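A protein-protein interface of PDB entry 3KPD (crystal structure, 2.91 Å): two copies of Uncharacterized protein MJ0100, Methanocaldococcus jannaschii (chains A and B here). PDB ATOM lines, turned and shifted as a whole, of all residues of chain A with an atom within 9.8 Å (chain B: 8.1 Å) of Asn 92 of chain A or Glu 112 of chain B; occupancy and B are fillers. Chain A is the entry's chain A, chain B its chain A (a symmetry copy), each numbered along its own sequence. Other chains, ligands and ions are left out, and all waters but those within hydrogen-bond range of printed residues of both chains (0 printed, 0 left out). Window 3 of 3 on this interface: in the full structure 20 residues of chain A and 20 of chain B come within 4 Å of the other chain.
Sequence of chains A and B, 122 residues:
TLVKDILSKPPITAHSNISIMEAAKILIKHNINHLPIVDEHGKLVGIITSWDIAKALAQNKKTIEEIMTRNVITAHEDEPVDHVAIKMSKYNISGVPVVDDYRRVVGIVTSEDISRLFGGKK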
ATOM      1  N   ASN A  33     -32.636  22.027  20.846  1.00  0.00           N
ATOM      2  CA  ASN A  33     -32.642  22.002  19.391  1.00  0.00           C
ATOM      3  C   ASN A  33     -32.287  20.649  18.783  1.00  0.00           C
ATOM      4  O   ASN A  33     -32.128  20.548  17.575  1.00  0.00           O
ATOM      5  CB  ASN A  33     -31.753  23.093  18.807  1.00  0.00           C
ATOM      6  CG  ASN A  33     -32.007  23.316  17.326  1.00  0.00           C
ATOM      7  OD1 ASN A  33     -33.131  23.187  16.854  1.00  0.00           O
ATOM      8  ND2 ASN A  33     -30.964  23.645  16.589  1.00  0.00           N
ATOM      9  N   HIS A  34     -32.187  19.610  19.607  1.00  0.00           N
ATOM     10  CA  HIS A  34     -31.696  18.320  19.131  1.00  0.00           C
ATOM     11  C   HIS A  34     -32.525  17.224  19.697  1.00  0.00           C
ATOM     12  O   HIS A  34     -32.648  17.100  20.912  1.00  0.00           O
ATOM     13  CB  HIS A  34     -30.235  18.107  19.533  1.00  0.00           C
ATOM     14  CG  HIS A  34     -29.293  19.046  18.856  1.00  0.00           C
ATOM     15  ND1 HIS A  34     -28.979  20.283  19.371  1.00  0.00           N
ATOM     16  CD2 HIS A  34     -28.639  18.951  17.675  1.00  0.00           C
ATOM     17  CE1 HIS A  34     -28.145  20.896  18.549  1.00  0.00           C
ATOM     18  NE2 HIS A  34     -27.926  20.110  17.511  1.00  0.00           N
ATOM     19  N   THR A  49     -33.618  18.037  14.307  1.00  0.00           N
ATOM     20  CA  THR A  49     -33.396  19.357  14.877  1.00  0.00           C
ATOM     21  C   THR A  49     -34.382  20.288  14.194  1.00  0.00           C
ATOM     22  O   THR A  49     -34.916  19.939  13.148  1.00  0.00           O
ATOM     23  CB  THR A  49     -31.972  19.883  14.616  1.00  0.00           C
ATOM     24  OG1 THR A  49     -31.855  20.312  13.251  1.00  0.00           O
ATOM     25  CG2 THR A  49     -30.914  18.828  14.918  1.00  0.00           C
ATOM     26  N   TRP A  51     -34.249  22.423  12.180  1.00  0.00           N
ATOM     27  CA  TRP A  51     -34.004  22.551  10.758  1.00  0.00           C
ATOM     28  C   TRP A  51     -34.872  21.576   9.967  1.00  0.00           C
ATOM     29  O   TRP A  51     -35.490  21.952   8.969  1.00  0.00           O
ATOM     30  CB  TRP A  51     -32.541  22.295  10.456  1.00  0.00           C
ATOM     31  CG  TRP A  51     -32.284  22.204   8.994  1.00  0.00           C
ATOM     32  CD1 TRP A  51     -32.263  21.067   8.220  1.00  0.00           C
ATOM     33  CD2 TRP A  51     -32.046  23.295   8.106  1.00  0.00           C
ATOM     34  NE1 TRP A  51     -32.012  21.397   6.911  1.00  0.00           N
ATOM     35  CE2 TRP A  51     -31.865  22.757   6.819  1.00  0.00           C
ATOM     36  CE3 TRP A  51     -31.947  24.676   8.282  1.00  0.00           C
ATOM     37  CZ2 TRP A  51     -31.585  23.544   5.728  1.00  0.00           C
ATOM     38  CZ3 TRP A  51     -31.684  25.452   7.197  1.00  0.00           C
ATOM     39  CH2 TRP A  51     -31.508  24.889   5.934  1.00  0.00           C
ATOM     40  N   ILE A  73     -23.951  11.902  13.583  1.00  0.00           N
ATOM     41  CA  ILE A  73     -22.597  12.018  14.116  1.00  0.00           C
ATOM     42  C   ILE A  73     -22.660  12.102  15.644  1.00  0.00           C
ATOM     43  O   ILE A  73     -23.371  12.939  16.194  1.00  0.00           O
ATOM     44  CB  ILE A  73     -21.873  13.252  13.506  1.00  0.00           C
ATOM     45  CG1 ILE A  73     -21.618  13.047  12.016  1.00  0.00           C
ATOM     46  CG2 ILE A  73     -20.519  13.502  14.146  1.00  0.00           C
ATOM     47  CD1 ILE A  73     -22.735  13.541  11.077  1.00  0.00           C
ATOM     48  N   VAL A  84     -14.558  16.895  20.452  1.00  0.00           N
ATOM     49  CA  VAL A  84     -15.953  16.960  20.011  1.00  0.00           C
ATOM     50  C   VAL A  84     -16.264  18.351  19.463  1.00  0.00           C
ATOM     51  O   VAL A  84     -16.970  18.473  18.469  1.00  0.00           O
ATOM     52  CB  VAL A  84     -16.933  16.594  21.154  1.00  0.00           C
ATOM     53  CG1 VAL A  84     -18.368  16.551  20.637  1.00  0.00           C
ATOM     54  CG2 VAL A  84     -16.540  15.265  21.782  1.00  0.00           C
ATOM     55  N   ALA A  85     -15.719  19.377  20.120  1.00  0.00           N
ATOM     56  CA  ALA A  85     -15.739  20.758  19.633  1.00  0.00           C
ATOM     57  C   ALA A  85     -15.296  20.851  18.159  1.00  0.00           C
ATOM     58  O   ALA A  85     -16.068  21.282  17.285  1.00  0.00           O
ATOM     59  CB  ALA A  85     -14.864  21.644  20.531  1.00  0.00           C
ATOM     60  N   ILE A  86     -14.060  20.406  17.908  1.00  0.00           N
ATOM     61  CA  ILE A  86     -13.476  20.261  16.571  1.00  0.00           C
ATOM     62  C   ILE A  86     -14.405  19.498  15.621  1.00  0.00           C
ATOM     63  O   ILE A  86     -14.497  19.821  14.435  1.00  0.00           O
ATOM     64  CB  ILE A  86     -12.046  19.602  16.665  1.00  0.00           C
ATOM     65  CG1 ILE A  86     -11.072  20.563  17.365  1.00  0.00           C
ATOM     66  CG2 ILE A  86     -11.473  19.247  15.282  1.00  0.00           C
ATOM     67  CD1 ILE A  86     -10.035  19.939  18.278  1.00  0.00           C
ATOM     68  N   LYS A  87     -15.118  18.509  16.146  1.00  0.00           N
ATOM     69  CA  LYS A  87     -15.901  17.621  15.304  1.00  0.00           C
ATOM     70  C   LYS A  87     -17.160  18.307  14.756  1.00  0.00           C
ATOM     71  O   LYS A  87     -17.506  18.159  13.566  1.00  0.00           O
ATOM     72  CB  LYS A  87     -16.247  16.345  16.074  1.00  0.00           C
ATOM     73  CG  LYS A  87     -16.569  15.136  15.185  1.00  0.00           C
ATOM     74  CD  LYS A  87     -17.311  14.038  15.946  1.00  0.00           C
ATOM     75  CE  LYS A  87     -16.392  13.237  16.872  1.00  0.00           C
ATOM     76  NZ  LYS A  87     -17.161  12.336  17.797  1.00  0.00           N
ATOM     77  N   MET A  88     -17.816  19.075  15.627  1.00  0.00           N
ATOM     78  CA  MET A  88     -19.059  19.769  15.304  1.00  0.00           C
ATOM     79  C   MET A  88     -18.840  20.939  14.358  1.00  0.00           C
ATOM     80  O   MET A  88     -19.683  21.208  13.487  1.00  0.00           O
ATOM     81  CB  MET A  88     -19.724  20.265  16.576  1.00  0.00           C
ATOM     82  CG  MET A  88     -20.268  19.153  17.454  1.00  0.00           C
ATOM     83  SD  MET A  88     -20.882  19.807  19.009  1.00  0.00           S
ATOM     84  CE  MET A  88     -19.415  20.571  19.691  1.00  0.00           C
ATOM     85  N   SER A  89     -17.723  21.647  14.529  1.00  0.00           N
ATOM     86  CA  SER A  89     -17.387  22.707  13.579  1.00  0.00           C
ATOM     87  C   SER A  89     -17.110  22.094  12.217  1.00  0.00           C
ATOM     88  O   SER A  89     -17.842  22.371  11.275  1.00  0.00           O
ATOM     89  CB  SER A  89     -16.261  23.648  14.058  1.00  0.00           C
ATOM     90  OG  SER A  89     -15.384  23.046  14.992  1.00  0.00           O
ATOM     91  N   LYS A  90     -16.117  21.211  12.141  1.00  0.00           N
ATOM     92  CA  LYS A  90     -15.761  20.539  10.886  1.00  0.00           C
ATOM     93  C   LYS A  90     -16.952  19.914  10.119  1.00  0.00           C
ATOM     94  O   LYS A  90     -16.873  19.691   8.903  1.00  0.00           O
ATOM     95  CB  LYS A  90     -14.641  19.508  11.139  1.00  0.00           C
ATOM     96  CG  LYS A  90     -14.376  18.496  10.003  1.00  0.00           C
ATOM     97  CD  LYS A  90     -13.139  17.623  10.321  1.00  0.00           C
ATOM     98  CE  LYS A  90     -13.036  16.369   9.416  1.00  0.00           C
ATOM     99  NZ  LYS A  90     -11.851  15.544   9.791  1.00  0.00           N
ATOM    100  N   TYR A  91     -18.048  19.638  10.821  1.00  0.00           N
ATOM    101  CA  TYR A  91     -19.215  19.030  10.196  1.00  0.00           C
ATOM    102  C   TYR A  91     -20.401  19.965  10.261  1.00  0.00           C
ATOM    103  O   TYR A  91     -21.499  19.652   9.764  1.00  0.00           O
ATOM    104  CB  TYR A  91     -19.541  17.703  10.879  1.00  0.00           C
ATOM    105  CG  TYR A  91     -18.741  16.546  10.342  1.00  0.00           C
ATOM    106  CD1 TYR A  91     -19.217  15.803   9.249  1.00  0.00           C
ATOM    107  CD2 TYR A  91     -17.502  16.212  10.897  1.00  0.00           C
ATOM    108  CE1 TYR A  91     -18.490  14.753   8.727  1.00  0.00           C
ATOM    109  CE2 TYR A  91     -16.766  15.163  10.388  1.00  0.00           C
ATOM    110  CZ  TYR A  91     -17.265  14.433   9.304  1.00  0.00           C
ATOM    111  OH  TYR A  91     -16.543  13.388   8.786  1.00  0.00           O
ATOM    112  N   ASN A  92     -20.140  21.115  10.891  1.00  0.00           N
ATOM    113  CA  ASN A  92     -21.090  22.207  11.065  1.00  0.00           C
ATOM    114  C   ASN A  92     -22.445  21.789  11.608  1.00  0.00           C
ATOM    115  O   ASN A  92     -23.480  21.850  10.927  1.00  0.00           O
ATOM    116  CB  ASN A  92     -21.166  23.096   9.825  1.00  0.00           C
ATOM    117  CG  ASN A  92     -20.292  24.337   9.971  1.00  0.00           C
ATOM    118  OD1 ASN A  92     -19.436  24.627   9.115  1.00  0.00           O
ATOM    119  ND2 ASN A  92     -20.486  25.067  11.083  1.00  0.00           N
ATOM    120  N   ILE A  93     -22.389  21.341  12.855  1.00  0.00           N
ATOM    121  CA  ILE A  93     -23.530  20.890  13.619  1.00  0.00           C
ATOM    122  C   ILE A  93     -23.255  21.342  15.049  1.00  0.00           C
ATOM    123  O   ILE A  93     -22.092  21.570  15.435  1.00  0.00           O
ATOM    124  CB  ILE A  93     -23.694  19.357  13.580  1.00  0.00           C
ATOM    125  CG1 ILE A  93     -22.363  18.651  13.819  1.00  0.00           C
ATOM    126  CG2 ILE A  93     -24.274  18.908  12.252  1.00  0.00           C
ATOM    127  CD1 ILE A  93     -22.529  17.231  14.272  1.00  0.00           C
ATOM    128  N   SER A  94     -24.315  21.483  15.835  1.00  0.00           N
ATOM    129  CA  SER A  94     -24.164  22.092  17.138  1.00  0.00           C
ATOM    130  C   SER A  94     -24.398  21.117  18.271  1.00  0.00           C
ATOM    131  O   SER A  94     -24.293  21.490  19.441  1.00  0.00           O
ATOM    132  CB  SER A  94     -25.060  23.321  17.256  1.00  0.00           C
ATOM    133  OG  SER A  94     -26.167  23.186  16.396  1.00  0.00           O
ATOM    134  N   GLY A  95     -24.702  19.870  17.924  1.00  0.00           N
ATOM    135  CA  GLY A  95     -25.035  18.865  18.931  1.00  0.00           C
ATOM    136  C   GLY A  95     -24.783  17.433  18.532  1.00  0.00           C
ATOM    137  O   GLY A  95     -25.087  17.019  17.421  1.00  0.00           O
ATOM    138  N   VAL A  96     -24.222  16.669  19.449  1.00  0.00           N
ATOM    139  CA  VAL A  96     -24.072  15.246  19.241  1.00  0.00           C
ATOM    140  C   VAL A  96     -24.680  14.441  20.371  1.00  0.00           C
ATOM    141  O   VAL A  96     -24.460  14.763  21.535  1.00  0.00           O
ATOM    142  CB  VAL A  96     -22.601  14.852  19.133  1.00  0.00           C
ATOM    143  CG1 VAL A  96     -22.045  15.317  17.815  1.00  0.00           C
ATOM    144  CG2 VAL A  96     -21.795  15.419  20.300  1.00  0.00           C
ATOM    145  N   SER A 111     -22.790  22.632  21.630  1.00  0.00           N
ATOM    146  CA  SER A 111     -21.821  23.737  21.743  1.00  0.00           C
ATOM    147  C   SER A 111     -22.214  24.651  22.903  1.00  0.00           C
ATOM    148  O   SER A 111     -21.364  25.169  23.617  1.00  0.00           O
ATOM    149  CB  SER A 111     -21.672  24.505  20.419  1.00  0.00           C
ATOM    150  OG  SER A 111     -22.921  24.681  19.764  1.00  0.00           O
ATOM    151  N   ILE B   6     -15.219  38.527   6.013  1.00  0.00           N
ATOM    152  CA  ILE B   6     -15.554  37.155   6.330  1.00  0.00           C
ATOM    153  C   ILE B   6     -17.029  36.956   6.007  1.00  0.00           C
ATOM    154  O   ILE B   6     -17.431  35.882   5.546  1.00  0.00           O
ATOM    155  CB  ILE B   6     -15.239  36.849   7.828  1.00  0.00           C
ATOM    156  CG1 ILE B   6     -13.793  36.384   7.977  1.00  0.00           C
ATOM    157  CG2 ILE B   6     -16.139  35.780   8.411  1.00  0.00           C
ATOM    158  CD1 ILE B   6     -12.752  37.526   8.070  1.00  0.00           C
ATOM    159  N   SER B   8     -21.000  36.901   4.795  1.00  0.00           N
ATOM    160  CA  SER B   8     -21.742  36.463   3.613  1.00  0.00           C
ATOM    161  C   SER B   8     -22.416  37.631   2.893  1.00  0.00           C
ATOM    162  O   SER B   8     -23.198  38.404   3.447  1.00  0.00           O
ATOM    163  CB  SER B   8     -22.708  35.331   3.943  1.00  0.00           C
ATOM    164  OG  SER B   8     -21.978  34.181   4.319  1.00  0.00           O
ATOM    165  N   ASN B  31     -30.022  27.185   1.738  1.00  0.00           N
ATOM    166  CA  ASN B  31     -29.301  26.341   2.682  1.00  0.00           C
ATOM    167  C   ASN B  31     -28.820  27.161   3.884  1.00  0.00           C
ATOM    168  O   ASN B  31     -27.709  26.991   4.373  1.00  0.00           O
ATOM    169  CB  ASN B  31     -28.132  25.620   1.991  1.00  0.00           C
ATOM    170  CG  ASN B  31     -27.598  24.471   2.812  1.00  0.00           C
ATOM    171  OD1 ASN B  31     -28.344  23.825   3.553  1.00  0.00           O
ATOM    172  ND2 ASN B  31     -26.301  24.216   2.699  1.00  0.00           N
ATOM    173  N   ILE B  32     -29.681  28.050   4.357  1.00  0.00           N
ATOM    174  CA  ILE B  32     -29.329  28.983   5.417  1.00  0.00           C
ATOM    175  C   ILE B  32     -30.157  28.746   6.676  1.00  0.00           C
ATOM    176  O   ILE B  32     -31.216  28.143   6.614  1.00  0.00           O
ATOM    177  CB  ILE B  32     -29.491  30.437   4.936  1.00  0.00           C
ATOM    178  CG1 ILE B  32     -30.911  30.655   4.408  1.00  0.00           C
ATOM    179  CG2 ILE B  32     -28.437  30.756   3.842  1.00  0.00           C
ATOM    180  CD1 ILE B  32     -31.430  32.062   4.655  1.00  0.00           C
ATOM    181  N   ASN B  33     -29.668  29.197   7.825  1.00  0.00           N
ATOM    182  CA  ASN B  33     -30.479  29.107   9.031  1.00  0.00           C
ATOM    183  C   ASN B  33     -30.876  30.454   9.626  1.00  0.00           C
ATOM    184  O   ASN B  33     -31.439  30.498  10.711  1.00  0.00           O
ATOM    185  CB  ASN B  33     -29.815  28.237  10.091  1.00  0.00           C
ATOM    186  CG  ASN B  33     -30.774  27.841  11.199  1.00  0.00           C
ATOM    187  OD1 ASN B  33     -31.961  27.643  10.964  1.00  0.00           O
ATOM    188  ND2 ASN B  33     -30.265  27.732  12.411  1.00  0.00           N
ATOM    189  N   HIS B  34     -30.608  31.545   8.914  1.00  0.00           N
ATOM    190  CA  HIS B  34     -30.807  32.876   9.479  1.00  0.00           C
ATOM    191  C   HIS B  34     -31.436  33.766   8.468  1.00  0.00           C
ATOM    192  O   HIS B  34     -30.898  33.949   7.381  1.00  0.00           O
ATOM    193  CB  HIS B  34     -29.478  33.485   9.931  1.00  0.00           C
ATOM    194  CG  HIS B  34     -28.861  32.768  11.086  1.00  0.00           C
ATOM    195  ND1 HIS B  34     -28.013  31.695  10.926  1.00  0.00           N
ATOM    196  CD2 HIS B  34     -29.015  32.934  12.420  1.00  0.00           C
ATOM    197  CE1 HIS B  34     -27.646  31.253  12.115  1.00  0.00           C
ATOM    198  NE2 HIS B  34     -28.242  31.985  13.038  1.00  0.00           N
ATOM    199  N   MET B  88     -21.497  35.412  20.081  1.00  0.00           N
ATOM    200  CA  MET B  88     -22.487  34.402  19.721  1.00  0.00           C
ATOM    201  C   MET B  88     -22.535  33.255  20.719  1.00  0.00           C
ATOM    202  O   MET B  88     -23.616  32.714  21.002  1.00  0.00           O
ATOM    203  CB  MET B  88     -22.191  33.853  18.336  1.00  0.00           C
ATOM    204  CG  MET B  88     -22.424  34.854  17.220  1.00  0.00           C
ATOM    205  SD  MET B  88     -21.891  34.189  15.640  1.00  0.00           S
ATOM    206  CE  MET B  88     -20.154  33.879  15.939  1.00  0.00           C
ATOM    207  N   ILE B  93     -26.081  31.847  20.050  1.00  0.00           N
ATOM    208  CA  ILE B  93     -26.684  32.051  18.752  1.00  0.00           C
ATOM    209  C   ILE B  93     -25.564  31.796  17.750  1.00  0.00           C
ATOM    210  O   ILE B  93     -24.369  31.902  18.085  1.00  0.00           O
ATOM    211  CB  ILE B  93     -27.227  33.483  18.576  1.00  0.00           C
ATOM    212  CG1 ILE B  93     -26.217  34.521  19.053  1.00  0.00           C
ATOM    213  CG2 ILE B  93     -28.532  33.664  19.326  1.00  0.00           C
ATOM    214  CD1 ILE B  93     -26.462  35.883  18.475  1.00  0.00           C
ATOM    215  N   SER B  94     -25.941  31.452  16.525  1.00  0.00           N
ATOM    216  CA  SER B  94     -24.949  31.005  15.572  1.00  0.00           C
ATOM    217  C   SER B  94     -24.760  31.972  14.423  1.00  0.00           C
ATOM    218  O   SER B  94     -23.939  31.732  13.537  1.00  0.00           O
ATOM    219  CB  SER B  94     -25.284  29.601  15.076  1.00  0.00           C
ATOM    220  OG  SER B  94     -26.672  29.382  15.174  1.00  0.00           O
ATOM    221  N   GLY B  95     -25.512  33.071  14.449  1.00  0.00           N
ATOM    222  CA  GLY B  95     -25.479  34.033  13.350  1.00  0.00           C
ATOM    223  C   GLY B  95     -25.863  35.446  13.708  1.00  0.00           C
ATOM    224  O   GLY B  95     -26.821  35.681  14.434  1.00  0.00           O
ATOM    225  N   VAL B 109     -22.683  37.050   9.408  1.00  0.00           N
ATOM    226  CA  VAL B 109     -21.646  36.099   9.788  1.00  0.00           C
ATOM    227  C   VAL B 109     -22.307  34.972  10.542  1.00  0.00           C
ATOM    228  O   VAL B 109     -23.132  35.195  11.417  1.00  0.00           O
ATOM    229  CB  VAL B 109     -20.565  36.703  10.723  1.00  0.00           C
ATOM    230  CG1 VAL B 109     -19.513  35.659  11.063  1.00  0.00           C
ATOM    231  CG2 VAL B 109     -19.879  37.891  10.093  1.00  0.00           C
ATOM    232  N   THR B 110     -21.935  33.751  10.212  1.00  0.00           N
ATOM    233  CA  THR B 110     -22.350  32.607  11.008  1.00  0.00           C
ATOM    234  C   THR B 110     -21.111  31.918  11.534  1.00  0.00           C
ATOM    235  O   THR B 110     -20.038  32.066  10.966  1.00  0.00           O
ATOM    236  CB  THR B 110     -23.131  31.639  10.170  1.00  0.00           C
ATOM    237  OG1 THR B 110     -22.355  31.293   9.023  1.00  0.00           O
ATOM    238  CG2 THR B 110     -24.398  32.295   9.696  1.00  0.00           C
ATOM    239  N   SER B 111     -21.249  31.184  12.631  1.00  0.00           N
ATOM    240  CA  SER B 111     -20.134  30.375  13.156  1.00  0.00           C
ATOM    241  C   SER B 111     -19.578  29.485  12.048  1.00  0.00           C
ATOM    242  O   SER B 111     -18.376  29.258  11.961  1.00  0.00           O
ATOM    243  CB  SER B 111     -20.548  29.569  14.399  1.00  0.00           C
ATOM    244  OG  SER B 111     -21.858  29.031  14.272  1.00  0.00           O
ATOM    245  N   GLU B 112     -20.475  29.039  11.174  1.00  0.00           N
ATOM    246  CA  GLU B 112     -20.119  28.353   9.935  1.00  0.00           C
ATOM    247  C   GLU B 112     -18.959  29.035   9.176  1.00  0.00           C
ATOM    248  O   GLU B 112     -18.151  28.351   8.571  1.00  0.00           O
ATOM    249  CB  GLU B 112     -21.352  28.214   9.031  1.00  0.00           C
ATOM    250  CG  GLU B 112     -22.432  27.210   9.518  1.00  0.00           C
ATOM    251  CD  GLU B 112     -23.594  27.834  10.327  1.00  0.00           C
ATOM    252  OE1 GLU B 112     -24.719  27.974   9.792  1.00  0.00           O
ATOM    253  OE2 GLU B 112     -23.386  28.166  11.515  1.00  0.00           O
ATOM    254  N   ASP B 113     -18.877  30.367   9.225  1.00  0.00           N
ATOM    255  CA  ASP B 113     -17.809  31.136   8.571  1.00  0.00           C
ATOM    256  C   ASP B 113     -16.593  31.271   9.492  1.00  0.00           C
ATOM    257  O   ASP B 113     -15.456  31.101   9.060  1.00  0.00           O
ATOM    258  CB  ASP B 113     -18.295  32.541   8.166  1.00  0.00           C
ATOM    259  CG  ASP B 113     -19.670  32.537   7.478  1.00  0.00           C
ATOM    260  OD1 ASP B 113     -19.814  31.907   6.410  1.00  0.00           O
ATOM    261  OD2 ASP B 113     -20.606  33.191   7.991  1.00  0.00           O
ATOM    262  N   ILE B 114     -16.851  31.588  10.760  1.00  0.00           N
ATOM    263  CA  ILE B 114     -15.819  31.718  11.788  1.00  0.00           C
ATOM    264  C   ILE B 114     -14.919  30.464  11.863  1.00  0.00           C
ATOM    265  O   ILE B 114     -13.707  30.556  12.116  1.00  0.00           O
ATOM    266  CB  ILE B 114     -16.459  31.973  13.172  1.00  0.00           C
ATOM    267  CG1 ILE B 114     -17.467  33.124  13.102  1.00  0.00           C
ATOM    268  CG2 ILE B 114     -15.401  32.214  14.245  1.00  0.00           C
ATOM    269  CD1 ILE B 114     -16.934  34.478  13.487  1.00  0.00           C
ATOM    270  N   SER B 115     -15.510  29.298  11.627  1.00  0.00           N
ATOM    271  CA  SER B 115     -14.807  28.024  11.653  1.00  0.00           C
ATOM    272  C   SER B 115     -14.122  27.713  10.318  1.00  0.00           C
ATOM    273  O   SER B 115     -14.219  26.582   9.813  1.00  0.00           O
ATOM    274  CB  SER B 115     -15.782  26.899  12.028  1.00  0.00           C
ATOM    275  OG  SER B 115     -16.784  26.716  11.033  1.00  0.00           O
ATOM    276  N   ARG B 116     -13.483  28.723   9.737  1.00  0.00           N
ATOM    277  CA  ARG B 116     -12.601  28.586   8.579  1.00  0.00           C
ATOM    278  C   ARG B 116     -11.433  29.476   8.965  1.00  0.00           C
ATOM    279  O   ARG B 116     -10.449  29.621   8.247  1.00  0.00           O
ATOM    280  CB  ARG B 116     -13.288  29.008   7.281  1.00  0.00           C
ATOM    281  CG  ARG B 116     -14.459  28.083   6.879  1.00  0.00           C
ATOM    282  CD  ARG B 116     -14.629  27.974   5.358  1.00  0.00           C
ATOM    283  NE  ARG B 116     -15.659  26.994   4.988  1.00  0.00           N
ATOM    284  CZ  ARG B 116     -16.781  27.268   4.316  1.00  0.00           C
ATOM    285  NH1 ARG B 116     -17.045  28.510   3.900  1.00  0.00           N
ATOM    286  NH2 ARG B 116     -17.641  26.290   4.042  1.00  0.00           N
ATOM    287  N   LEU B 117     -11.585  30.064  10.147  1.00  0.00           N
ATOM    288  CA  LEU B 117     -10.486  30.637  10.906  1.00  0.00           C
ATOM    289  C   LEU B 117     -10.047  29.660  12.013  1.00  0.00           C
ATOM    290  O   LEU B 117      -9.046  29.900  12.701  1.00  0.00           O
ATOM    291  CB  LEU B 117     -10.868  31.999  11.520  1.00  0.00           C
ATOM    292  CG  LEU B 117     -11.491  33.181  10.743  1.00  0.00           C
ATOM    293  CD1 LEU B 117     -11.285  34.453  11.552  1.00  0.00           C
ATOM    294  CD2 LEU B 117     -10.992  33.361   9.280  1.00  0.00           C
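Positions printed for both chains: 33, 34, 88, 93, 94, 95 and 111.
Hydrophobic or aromatic side chains of chain A that line the printed part of chain B: Trp 51.
Among the printed residues, no Asp or Glu carboxylate lies within 4 Å of a Lys or Arg side-chain nitrogen of the other chain.
Among the printed residues, merely in contact across the chains: Trp 51 of chain A with Ile 32 of chain B (2.8 Å), Asn 92 of chain A with Glu 112 of chain B (3.3 Å), Ser 89 of chain A with Ser 115 of chain B (3.9 Å), Asn 92 of chain A with Ser 115 of chain B (3.9 Å), Trp 51 of chain A with Asn 31 of chain B (3.9 Å) and Trp 51 of chain A with Asn 33 of chain B (3.9996 Å).
The side-chain hydroxyl (OG1) of Thr 49 of chain A lies close to the backbone NH (N) of Trp 51 of chain A, at 3.4 Å.
OG of Ser 89 of chain A sits at hydrogen-bond distance from O of Ala 85 of chain A (3.0 Å).
The backbone carbonyl oxygen (O) of Ile 86 of chain A lies within hydrogen-bond range of the side-chain hydroxyl (OG) of Ser 89 of chain A, at 3.4 Å.
The side-chain hydroxyl (OG) of Ser 111 of chain B lies within hydrogen-bond range of the side-chain carboxylate (OE2) of Glu 112 of chain B (3.3 Å).
O of Ser 111 of chain B sits at hydrogen-bond distance from OG of Ser 115 of chain B, 3.1 Å away.
The backbone carbonyl oxygen (O) of Glu 112 of chain B lies within hydrogen-bond range of the side-chain hydroxyl (OG) of Ser 115 of chain B, 3.3 Å away.
Ala 85 of chain A touches none of the printed residues of chain B.
Of the printed residues of chain B, Ser 89 of chain A touches Ser 115.
Of the printed residues of chain B, Asn 92 of chain A touches Glu 112 and Ser 115.
Printed residues of chain A within 4 Å of Ile 32 of chain B: Trp 51.
Printed residues of chain A within 4 Å of Asn 33 of chain B: Trp 51 (3.9996 Å).
Thr 110 of chain B touches none of the printed residues of chain A.
No residue of chain A comes within 4 Å of Ser 111 of chain B.
Glu 112 of chain B touches just one residue of chain A: Asn 92 (3.3 Å).
The nearest printed residue of chain B that does not touch Asn 92 of chain A is Ser 111 of chain B (4.6 Å).
The nearest residue of chain A that does not touch Glu 112 of chain B is Ser 89 of chain A (6.5 Å).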
